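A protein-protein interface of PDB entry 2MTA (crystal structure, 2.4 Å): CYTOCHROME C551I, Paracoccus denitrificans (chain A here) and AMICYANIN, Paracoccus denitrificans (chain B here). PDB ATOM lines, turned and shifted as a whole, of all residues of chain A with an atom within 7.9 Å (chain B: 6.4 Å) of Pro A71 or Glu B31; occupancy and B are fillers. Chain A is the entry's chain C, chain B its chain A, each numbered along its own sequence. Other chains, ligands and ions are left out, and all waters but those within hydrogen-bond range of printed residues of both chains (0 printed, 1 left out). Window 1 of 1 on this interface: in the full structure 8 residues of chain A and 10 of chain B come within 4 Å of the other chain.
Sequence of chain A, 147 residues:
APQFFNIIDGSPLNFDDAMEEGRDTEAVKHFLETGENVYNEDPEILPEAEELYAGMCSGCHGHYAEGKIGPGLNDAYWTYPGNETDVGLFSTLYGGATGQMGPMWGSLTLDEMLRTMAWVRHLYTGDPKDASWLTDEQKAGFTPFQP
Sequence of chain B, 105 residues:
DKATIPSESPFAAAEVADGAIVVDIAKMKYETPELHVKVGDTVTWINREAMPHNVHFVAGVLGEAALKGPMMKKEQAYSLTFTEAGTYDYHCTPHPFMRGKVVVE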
ATOM      1  N   TYR A  53      13.041   8.068  -7.266  1.00  0.00           N
ATOM      2  CA  TYR A  53      12.102   9.026  -6.723  1.00  0.00           C
ATOM      3  C   TYR A  53      12.843  10.269  -6.270  1.00  0.00           C
ATOM      4  O   TYR A  53      12.538  11.371  -6.735  1.00  0.00           O
ATOM      5  CB  TYR A  53      11.366   8.492  -5.531  1.00  0.00           C
ATOM      6  CG  TYR A  53      10.295   9.488  -5.078  1.00  0.00           C
ATOM      7  CD1 TYR A  53       9.083   9.530  -5.738  1.00  0.00           C
ATOM      8  CD2 TYR A  53      10.531  10.371  -4.039  1.00  0.00           C
ATOM      9  CE1 TYR A  53       8.129  10.438  -5.378  1.00  0.00           C
ATOM     10  CE2 TYR A  53       9.579  11.287  -3.667  1.00  0.00           C
ATOM     11  CZ  TYR A  53       8.383  11.310  -4.353  1.00  0.00           C
ATOM     12  OH  TYR A  53       7.429  12.252  -4.049  1.00  0.00           O
ATOM     13  N   CYS A  57      11.634  13.347  -8.359  1.00  0.00           N
ATOM     14  CA  CYS A  57      10.285  13.662  -7.996  1.00  0.00           C
ATOM     15  C   CYS A  57      10.174  14.421  -6.729  1.00  0.00           C
ATOM     16  O   CYS A  57       9.321  15.279  -6.629  1.00  0.00           O
ATOM     17  CB  CYS A  57       9.478  12.400  -7.845  1.00  0.00           C
ATOM     18  SG  CYS A  57       9.598  11.050  -9.077  1.00  0.00           S
ATOM     19  N   CYS A  60       9.302  18.621  -6.528  1.00  0.00           N
ATOM     20  CA  CYS A  60       7.963  19.077  -6.562  1.00  0.00           C
ATOM     21  C   CYS A  60       7.067  18.340  -5.610  1.00  0.00           C
ATOM     22  O   CYS A  60       6.276  19.000  -4.948  1.00  0.00           O
ATOM     23  CB  CYS A  60       7.559  18.906  -7.960  1.00  0.00           C
ATOM     24  SG  CYS A  60       8.734  19.865  -8.924  1.00  0.00           S
ATOM     25  N   HIS A  61       7.102  17.025  -5.438  1.00  0.00           N
ATOM     26  CA  HIS A  61       6.166  16.309  -4.553  1.00  0.00           C
ATOM     27  C   HIS A  61       6.589  16.055  -3.144  1.00  0.00           C
ATOM     28  O   HIS A  61       5.861  15.530  -2.280  1.00  0.00           O
ATOM     29  CB  HIS A  61       5.811  14.985  -5.102  1.00  0.00           C
ATOM     30  CG  HIS A  61       5.179  15.213  -6.434  1.00  0.00           C
ATOM     31  ND1 HIS A  61       3.863  15.576  -6.477  1.00  0.00           N
ATOM     32  CD2 HIS A  61       5.693  15.013  -7.726  1.00  0.00           C
ATOM     33  CE1 HIS A  61       3.553  15.508  -7.795  1.00  0.00           C
ATOM     34  NE2 HIS A  61       4.555  15.194  -8.543  1.00  0.00           N
ATOM     35  N   GLY A  62       7.772  16.509  -2.863  1.00  0.00           N
ATOM     36  CA  GLY A  62       8.330  16.255  -1.549  1.00  0.00           C
ATOM     37  C   GLY A  62       8.913  14.861  -1.386  1.00  0.00           C
ATOM     38  O   GLY A  62       8.704  13.883  -2.113  1.00  0.00           O
ATOM     39  N   ALA A  65       6.448  12.185  -0.898  1.00  0.00           N
ATOM     40  CA  ALA A  65       5.288  12.431  -1.751  1.00  0.00           C
ATOM     41  C   ALA A  65       4.037  12.854  -1.012  1.00  0.00           C
ATOM     42  O   ALA A  65       2.893  12.544  -1.334  1.00  0.00           O
ATOM     43  CB  ALA A  65       4.969  11.177  -2.615  1.00  0.00           C
ATOM     44  N   GLU A  66       4.301  13.664  -0.004  1.00  0.00           N
ATOM     45  CA  GLU A  66       3.283  14.237   0.830  1.00  0.00           C
ATOM     46  C   GLU A  66       2.875  15.591   0.208  1.00  0.00           C
ATOM     47  O   GLU A  66       1.830  16.125   0.572  1.00  0.00           O
ATOM     48  CB  GLU A  66       3.822  14.383   2.266  1.00  0.00           C
ATOM     49  CG  GLU A  66       4.746  15.527   2.677  1.00  0.00           C
ATOM     50  CD  GLU A  66       6.254  15.375   2.474  1.00  0.00           C
ATOM     51  OE1 GLU A  66       6.665  14.883   1.446  1.00  0.00           O
ATOM     52  OE2 GLU A  66       7.048  15.771   3.327  1.00  0.00           O
ATOM     53  N   GLY A  67       3.627  16.174  -0.763  1.00  0.00           N
ATOM     54  CA  GLY A  67       3.229  17.353  -1.527  1.00  0.00           C
ATOM     55  C   GLY A  67       4.178  18.462  -1.281  1.00  0.00           C
ATOM     56  O   GLY A  67       4.737  18.496  -0.187  1.00  0.00           O
ATOM     57  N   LYS A  68       4.439  19.354  -2.239  1.00  0.00           N
ATOM     58  CA  LYS A  68       5.203  20.573  -1.992  1.00  0.00           C
ATOM     59  C   LYS A  68       4.766  21.514  -3.116  1.00  0.00           C
ATOM     60  O   LYS A  68       3.668  22.050  -3.052  1.00  0.00           O
ATOM     61  CB  LYS A  68       6.694  20.330  -2.077  1.00  0.00           C
ATOM     62  CG  LYS A  68       7.369  21.425  -1.265  1.00  0.00           C
ATOM     63  CD  LYS A  68       8.703  21.907  -1.807  1.00  0.00           C
ATOM     64  CE  LYS A  68       9.673  20.755  -1.944  1.00  0.00           C
ATOM     65  NZ  LYS A  68       9.781  19.987  -0.710  1.00  0.00           N
ATOM     66  N   ILE A  69       5.541  21.764  -4.158  1.00  0.00           N
ATOM     67  CA  ILE A  69       5.151  22.576  -5.307  1.00  0.00           C
ATOM     68  C   ILE A  69       3.920  21.936  -5.964  1.00  0.00           C
ATOM     69  O   ILE A  69       2.988  22.589  -6.418  1.00  0.00           O
ATOM     70  CB  ILE A  69       6.403  22.604  -6.264  1.00  0.00           C
ATOM     71  CG1 ILE A  69       7.336  23.753  -5.945  1.00  0.00           C
ATOM     72  CG2 ILE A  69       5.957  22.749  -7.709  1.00  0.00           C
ATOM     73  CD1 ILE A  69       7.605  24.074  -4.463  1.00  0.00           C
ATOM     74  N   GLY A  70       3.996  20.635  -6.166  1.00  0.00           N
ATOM     75  CA  GLY A  70       2.910  19.892  -6.792  1.00  0.00           C
ATOM     76  C   GLY A  70       2.188  19.048  -5.736  1.00  0.00           C
ATOM     77  O   GLY A  70       2.554  19.098  -4.547  1.00  0.00           O
ATOM     78  N   PRO A  71       1.185  18.256  -6.057  1.00  0.00           N
ATOM     79  CA  PRO A  71       0.338  17.577  -5.060  1.00  0.00           C
ATOM     80  C   PRO A  71       0.885  16.357  -4.305  1.00  0.00           C
ATOM     81  O   PRO A  71       1.855  15.726  -4.697  1.00  0.00           O
ATOM     82  CB  PRO A  71      -0.933  17.199  -5.825  1.00  0.00           C
ATOM     83  CG  PRO A  71      -0.449  17.035  -7.255  1.00  0.00           C
ATOM     84  CD  PRO A  71       0.640  18.105  -7.391  1.00  0.00           C
ATOM     85  N   GLY A  72       0.272  15.906  -3.234  1.00  0.00           N
ATOM     86  CA  GLY A  72       0.657  14.692  -2.592  1.00  0.00           C
ATOM     87  C   GLY A  72       0.144  13.580  -3.456  1.00  0.00           C
ATOM     88  O   GLY A  72      -0.864  13.670  -4.141  1.00  0.00           O
ATOM     89  N   LEU A  73       1.015  12.588  -3.434  1.00  0.00           N
ATOM     90  CA  LEU A  73       0.864  11.318  -4.115  1.00  0.00           C
ATOM     91  C   LEU A  73       0.689  10.240  -3.040  1.00  0.00           C
ATOM     92  O   LEU A  73       0.691   9.056  -3.368  1.00  0.00           O
ATOM     93  CB  LEU A  73       2.116  11.054  -4.910  1.00  0.00           C
ATOM     94  CG  LEU A  73       2.504  11.720  -6.202  1.00  0.00           C
ATOM     95  CD1 LEU A  73       1.697  12.939  -6.563  1.00  0.00           C
ATOM     96  CD2 LEU A  73       3.899  12.137  -6.030  1.00  0.00           C
ATOM     97  N   ASN A  74       0.531  10.570  -1.752  1.00  0.00           N
ATOM     98  CA  ASN A  74       0.478   9.538  -0.739  1.00  0.00           C
ATOM     99  C   ASN A  74      -0.831   9.076  -0.103  1.00  0.00           C
ATOM    100  O   ASN A  74      -0.788   8.462   0.956  1.00  0.00           O
ATOM    101  CB  ASN A  74       1.458   9.912   0.394  1.00  0.00           C
ATOM    102  CG  ASN A  74       1.130  11.045   1.331  1.00  0.00           C
ATOM    103  OD1 ASN A  74       0.148  11.724   1.106  1.00  0.00           O
ATOM    104  ND2 ASN A  74       1.880  11.403   2.377  1.00  0.00           N
ATOM    105  N   ASP A  75      -2.010   9.203  -0.681  1.00  0.00           N
ATOM    106  CA  ASP A  75      -3.238   8.822  -0.025  1.00  0.00           C
ATOM    107  C   ASP A  75      -4.110   8.407  -1.182  1.00  0.00           C
ATOM    108  O   ASP A  75      -3.719   8.346  -2.350  1.00  0.00           O
ATOM    109  CB  ASP A  75      -3.895  10.014   0.756  1.00  0.00           C
ATOM    110  CG  ASP A  75      -4.060  11.352   0.013  1.00  0.00           C
ATOM    111  OD1 ASP A  75      -4.213  11.403  -1.220  1.00  0.00           O
ATOM    112  OD2 ASP A  75      -4.030  12.388   0.683  1.00  0.00           O
ATOM    113  N   ALA A  76      -5.354   8.194  -0.840  1.00  0.00           N
ATOM    114  CA  ALA A  76      -6.288   7.732  -1.809  1.00  0.00           C
ATOM    115  C   ALA A  76      -6.955   8.755  -2.683  1.00  0.00           C
ATOM    116  O   ALA A  76      -7.871   8.403  -3.422  1.00  0.00           O
ATOM    117  CB  ALA A  76      -7.338   6.966  -1.058  1.00  0.00           C
ATOM    118  N   TYR A  77      -6.628  10.038  -2.633  1.00  0.00           N
ATOM    119  CA  TYR A  77      -7.291  10.958  -3.534  1.00  0.00           C
ATOM    120  C   TYR A  77      -6.268  11.205  -4.638  1.00  0.00           C
ATOM    121  O   TYR A  77      -5.136  11.568  -4.368  1.00  0.00           O
ATOM    122  CB  TYR A  77      -7.676  12.293  -2.800  1.00  0.00           C
ATOM    123  CG  TYR A  77      -8.283  13.329  -3.771  1.00  0.00           C
ATOM    124  CD1 TYR A  77      -9.486  13.079  -4.410  1.00  0.00           C
ATOM    125  CD2 TYR A  77      -7.529  14.431  -4.162  1.00  0.00           C
ATOM    126  CE1 TYR A  77      -9.930  13.893  -5.451  1.00  0.00           C
ATOM    127  CE2 TYR A  77      -7.969  15.239  -5.200  1.00  0.00           C
ATOM    128  CZ  TYR A  77      -9.157  14.961  -5.868  1.00  0.00           C
ATOM    129  OH  TYR A  77      -9.472  15.626  -7.046  1.00  0.00           O
ATOM    130  N   TRP A  78      -6.712  11.076  -5.876  1.00  0.00           N
ATOM    131  CA  TRP A  78      -5.933  11.283  -7.050  1.00  0.00           C
ATOM    132  C   TRP A  78      -6.729  12.246  -7.889  1.00  0.00           C
ATOM    133  O   TRP A  78      -7.900  12.004  -8.221  1.00  0.00           O
ATOM    134  CB  TRP A  78      -5.724   9.949  -7.786  1.00  0.00           C
ATOM    135  CG  TRP A  78      -4.470   9.244  -7.270  1.00  0.00           C
ATOM    136  CD1 TRP A  78      -3.159   9.690  -7.438  1.00  0.00           C
ATOM    137  CD2 TRP A  78      -4.529   8.151  -6.492  1.00  0.00           C
ATOM    138  NE1 TRP A  78      -2.407   8.870  -6.728  1.00  0.00           N
ATOM    139  CE2 TRP A  78      -3.211   7.944  -6.155  1.00  0.00           C
ATOM    140  CE3 TRP A  78      -5.551   7.387  -6.041  1.00  0.00           C
ATOM    141  CZ2 TRP A  78      -2.890   6.907  -5.330  1.00  0.00           C
ATOM    142  CZ3 TRP A  78      -5.217   6.342  -5.200  1.00  0.00           C
ATOM    143  CH2 TRP A  78      -3.900   6.101  -4.844  1.00  0.00           C
ATOM    144  N   THR A  79      -6.120  13.362  -8.230  1.00  0.00           N
ATOM    145  CA  THR A  79      -6.713  14.347  -9.106  1.00  0.00           C
ATOM    146  C   THR A  79      -7.129  13.690 -10.403  1.00  0.00           C
ATOM    147  O   THR A  79      -8.056  14.107 -11.075  1.00  0.00           O
ATOM    148  CB  THR A  79      -5.652  15.420  -9.297  1.00  0.00           C
ATOM    149  OG1 THR A  79      -5.399  15.934  -7.991  1.00  0.00           O
ATOM    150  CG2 THR A  79      -6.041  16.515 -10.213  1.00  0.00           C
ATOM    151  N   TYR A  80      -6.424  12.686 -10.849  1.00  0.00           N
ATOM    152  CA  TYR A  80      -6.829  11.998 -12.037  1.00  0.00           C
ATOM    153  C   TYR A  80      -7.203  10.626 -11.443  1.00  0.00           C
ATOM    154  O   TYR A  80      -6.445   9.922 -10.756  1.00  0.00           O
ATOM    155  CB  TYR A  80      -5.640  12.060 -12.911  1.00  0.00           C
ATOM    156  CG  TYR A  80      -5.333  13.475 -13.415  1.00  0.00           C
ATOM    157  CD1 TYR A  80      -6.035  13.973 -14.517  1.00  0.00           C
ATOM    158  CD2 TYR A  80      -4.346  14.249 -12.825  1.00  0.00           C
ATOM    159  CE1 TYR A  80      -5.744  15.225 -15.047  1.00  0.00           C
ATOM    160  CE2 TYR A  80      -4.053  15.510 -13.339  1.00  0.00           C
ATOM    161  CZ  TYR A  80      -4.746  15.992 -14.447  1.00  0.00           C
ATOM    162  OH  TYR A  80      -4.421  17.230 -15.007  1.00  0.00           O
ATOM    163  N   MET A 101       4.601  19.108 -14.983  1.00  0.00           N
ATOM    164  CA  MET A 101       4.574  17.681 -14.802  1.00  0.00           C
ATOM    165  C   MET A 101       4.540  17.234 -16.262  1.00  0.00           C
ATOM    166  O   MET A 101       3.450  16.969 -16.738  1.00  0.00           O
ATOM    167  CB  MET A 101       3.287  17.284 -14.062  1.00  0.00           C
ATOM    168  CG  MET A 101       3.211  15.785 -13.866  1.00  0.00           C
ATOM    169  SD  MET A 101       4.563  15.017 -12.884  1.00  0.00           S
ATOM    170  CE  MET A 101       4.243  13.427 -13.602  1.00  0.00           C
ATOM    171  N   VAL B  23      -6.496  23.669  -5.849  1.00  0.00           N
ATOM    172  CA  VAL B  23      -6.006  22.975  -4.692  1.00  0.00           C
ATOM    173  C   VAL B  23      -7.141  22.081  -4.200  1.00  0.00           C
ATOM    174  O   VAL B  23      -8.237  22.545  -3.888  1.00  0.00           O
ATOM    175  CB  VAL B  23      -5.636  23.992  -3.678  1.00  0.00           C
ATOM    176  CG1 VAL B  23      -5.202  23.339  -2.343  1.00  0.00           C
ATOM    177  CG2 VAL B  23      -4.500  24.800  -4.275  1.00  0.00           C
ATOM    178  N   ASP B  24      -6.935  20.773  -4.152  1.00  0.00           N
ATOM    179  CA  ASP B  24      -7.987  19.896  -3.722  1.00  0.00           C
ATOM    180  C   ASP B  24      -7.908  19.715  -2.240  1.00  0.00           C
ATOM    181  O   ASP B  24      -6.801  19.805  -1.648  1.00  0.00           O
ATOM    182  CB  ASP B  24      -7.865  18.574  -4.461  1.00  0.00           C
ATOM    183  CG  ASP B  24      -8.193  18.715  -5.947  1.00  0.00           C
ATOM    184  OD1 ASP B  24      -9.305  19.112  -6.287  1.00  0.00           O
ATOM    185  OD2 ASP B  24      -7.352  18.425  -6.784  1.00  0.00           O
ATOM    186  N   ILE B  25      -9.060  19.547  -1.585  1.00  0.00           N
ATOM    187  CA  ILE B  25      -8.939  19.388  -0.169  1.00  0.00           C
ATOM    188  C   ILE B  25      -9.521  18.044  -0.040  1.00  0.00           C
ATOM    189  O   ILE B  25     -10.650  17.796  -0.444  1.00  0.00           O
ATOM    190  CB  ILE B  25      -9.770  20.400   0.596  1.00  0.00           C
ATOM    191  CG1 ILE B  25      -9.349  21.825   0.247  1.00  0.00           C
ATOM    192  CG2 ILE B  25      -9.550  20.197   2.067  1.00  0.00           C
ATOM    193  CD1 ILE B  25     -10.427  22.734   0.845  1.00  0.00           C
ATOM    194  N   ALA B  26      -8.736  17.149   0.485  1.00  0.00           N
ATOM    195  CA  ALA B  26      -9.215  15.816   0.689  1.00  0.00           C
ATOM    196  C   ALA B  26      -8.328  15.180   1.762  1.00  0.00           C
ATOM    197  O   ALA B  26      -7.267  15.696   2.121  1.00  0.00           O
ATOM    198  CB  ALA B  26      -9.112  15.078  -0.625  1.00  0.00           C
ATOM    199  N   LYS B  27      -8.863  14.122   2.381  1.00  0.00           N
ATOM    200  CA  LYS B  27      -8.213  13.364   3.438  1.00  0.00           C
ATOM    201  C   LYS B  27      -7.588  14.256   4.471  1.00  0.00           C
ATOM    202  O   LYS B  27      -6.407  14.149   4.759  1.00  0.00           O
ATOM    203  CB  LYS B  27      -7.114  12.403   2.869  1.00  0.00           C
ATOM    204  CG  LYS B  27      -7.626  11.306   1.959  1.00  0.00           C
ATOM    205  CD  LYS B  27      -8.453  10.301   2.798  1.00  0.00           C
ATOM    206  CE  LYS B  27      -9.876  10.048   2.278  1.00  0.00           C
ATOM    207  NZ  LYS B  27     -10.806  11.179   2.468  1.00  0.00           N
ATOM    208  N   MET B  28      -8.413  15.172   4.979  1.00  0.00           N
ATOM    209  CA  MET B  28      -8.034  16.174   5.980  1.00  0.00           C
ATOM    210  C   MET B  28      -6.817  16.962   5.589  1.00  0.00           C
ATOM    211  O   MET B  28      -6.061  17.406   6.461  1.00  0.00           O
ATOM    212  CB  MET B  28      -7.806  15.505   7.325  1.00  0.00           C
ATOM    213  CG  MET B  28      -9.031  14.801   7.933  1.00  0.00           C
ATOM    214  SD  MET B  28     -10.374  15.905   8.462  1.00  0.00           S
ATOM    215  CE  MET B  28      -9.413  16.951   9.505  1.00  0.00           C
ATOM    216  N   LYS B  29      -6.579  17.188   4.292  1.00  0.00           N
ATOM    217  CA  LYS B  29      -5.504  18.088   3.974  1.00  0.00           C
ATOM    218  C   LYS B  29      -5.699  18.809   2.679  1.00  0.00           C
ATOM    219  O   LYS B  29      -6.544  18.445   1.865  1.00  0.00           O
ATOM    220  CB  LYS B  29      -4.195  17.343   3.923  1.00  0.00           C
ATOM    221  CG  LYS B  29      -4.027  16.324   2.825  1.00  0.00           C
ATOM    222  CD  LYS B  29      -2.588  15.839   2.877  1.00  0.00           C
ATOM    223  CE  LYS B  29      -2.525  14.422   2.402  1.00  0.00           C
ATOM    224  NZ  LYS B  29      -3.304  13.532   3.254  1.00  0.00           N
ATOM    225  N   TYR B  30      -4.885  19.854   2.600  1.00  0.00           N
ATOM    226  CA  TYR B  30      -4.696  20.677   1.417  1.00  0.00           C
ATOM    227  C   TYR B  30      -3.653  19.994   0.558  1.00  0.00           C
ATOM    228  O   TYR B  30      -2.438  20.122   0.785  1.00  0.00           O
ATOM    229  CB  TYR B  30      -4.160  22.037   1.741  1.00  0.00           C
ATOM    230  CG  TYR B  30      -5.140  22.862   2.543  1.00  0.00           C
ATOM    231  CD1 TYR B  30      -6.352  23.266   2.022  1.00  0.00           C
ATOM    232  CD2 TYR B  30      -4.812  23.206   3.830  1.00  0.00           C
ATOM    233  CE1 TYR B  30      -7.228  24.017   2.808  1.00  0.00           C
ATOM    234  CE2 TYR B  30      -5.670  23.956   4.605  1.00  0.00           C
ATOM    235  CZ  TYR B  30      -6.867  24.355   4.102  1.00  0.00           C
ATOM    236  OH  TYR B  30      -7.697  25.088   4.908  1.00  0.00           O
ATOM    237  N   GLU B  31      -4.131  19.328  -0.478  1.00  0.00           N
ATOM    238  CA  GLU B  31      -3.276  18.485  -1.266  1.00  0.00           C
ATOM    239  C   GLU B  31      -2.167  19.192  -1.998  1.00  0.00           C
ATOM    240  O   GLU B  31      -1.327  18.433  -2.446  1.00  0.00           O
ATOM    241  CB  GLU B  31      -4.086  17.661  -2.302  1.00  0.00           C
ATOM    242  CG  GLU B  31      -5.044  16.605  -1.779  1.00  0.00           C
ATOM    243  CD  GLU B  31      -4.422  15.324  -1.225  1.00  0.00           C
ATOM    244  OE1 GLU B  31      -3.461  14.832  -1.784  1.00  0.00           O
ATOM    245  OE2 GLU B  31      -4.918  14.757  -0.244  1.00  0.00           O
ATOM    246  N   THR B  32      -2.060  20.501  -2.165  1.00  0.00           N
ATOM    247  CA  THR B  32      -0.930  21.104  -2.800  1.00  0.00           C
ATOM    248  C   THR B  32      -0.569  22.219  -1.842  1.00  0.00           C
ATOM    249  O   THR B  32      -1.051  23.351  -1.961  1.00  0.00           O
ATOM    250  CB  THR B  32      -1.238  21.729  -4.142  1.00  0.00           C
ATOM    251  OG1 THR B  32      -1.760  20.707  -4.969  1.00  0.00           O
ATOM    252  CG2 THR B  32       0.028  22.309  -4.811  1.00  0.00           C
ATOM    253  N   PRO B  33       0.234  21.923  -0.804  1.00  0.00           N
ATOM    254  CA  PRO B  33       0.396  22.764   0.369  1.00  0.00           C
ATOM    255  C   PRO B  33       1.271  23.955   0.160  1.00  0.00           C
ATOM    256  O   PRO B  33       1.380  24.766   1.074  1.00  0.00           O
ATOM    257  CB  PRO B  33       0.934  21.806   1.410  1.00  0.00           C
ATOM    258  CG  PRO B  33       1.838  20.945   0.582  1.00  0.00           C
ATOM    259  CD  PRO B  33       0.951  20.650  -0.607  1.00  0.00           C
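Pro A71 touches two residues of chain B. Of chain A, only Pro A71 (3.2 Å), Gly A72 (3.1 Å) and Asp A75 (2.7 Å) come within 4 Å of Glu B31. Printed residues of chain B within 4 Å of Ile A69: Thr B32 (3.4 Å). Of the printed residues of chain A, Asp B24 touches Tyr A77 and Thr A79. Of the printed residues of chain B, Gly A67 touches Pro B33. The nearest residue of chain A that does not touch Glu B31 is Tyr A77 (4.1 Å).
The side-chain carboxylate (OD2) of Asp B24 sits at hydrogen-bond distance from the side-chain hydroxyl (OG1) of Thr A79 (3.4 Å). NZ of Lys B29 is in salt-bridge range of OD2 of Asp A75, 2.9 Å away. The backbone carbonyl oxygen (O) of Glu B31 is in hydrogen-bond range of the backbone NH (N) of Gly A72. The side-chain carboxylate of Glu B31 lies close to the side-chain carboxylate of Asp A75 (2.7 Å).
Hydrophobic or aromatic side chains of chain B within 4 Å of the printed part of chain A: Ala B26 and Pro B33.
The backbone NH (N) of Glu B31 sits at hydrogen-bond distance from the backbone carbonyl oxygen (O) of Asp B24 (3.0 Å). The backbone carbonyl oxygen (O) of Cys A60 sits close to the backbone NH (N) of Lys A68, 3.3 Å away. The backbone carbonyl oxygen (O) of Cys A60 sits at hydrogen-bond distance from the backbone NH (N) of Ile A69 (3.0 Å). The backbone carbonyl oxygen (O) of His A61 sits at hydrogen-bond distance from the backbone NH (N) of Gly A67, 2.8 Å away. ND1 of His A61 lies within hydrogen-bond range of O of Pro A71. The side-chain carboxylate (OD1) of Asp A75 is in hydrogen-bond range of the backbone NH (N) of Tyr A77 (3.1 Å).
Pro B33 touches Gly A67. Lys A68 touches Pro B33. Ile A69 touches Thr B32 (O to CG2, 3.4 Å). CA of Pro A71 touches O of Glu B31 (3.2 Å). Pro A71 touches Thr B32 (CB to OG1, 3.7 Å). Asp A75 touches Lys B27. Asp B24 touches Tyr A77. CG of Tyr A77 touches CB of Ala B26, 3.7 Å away.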
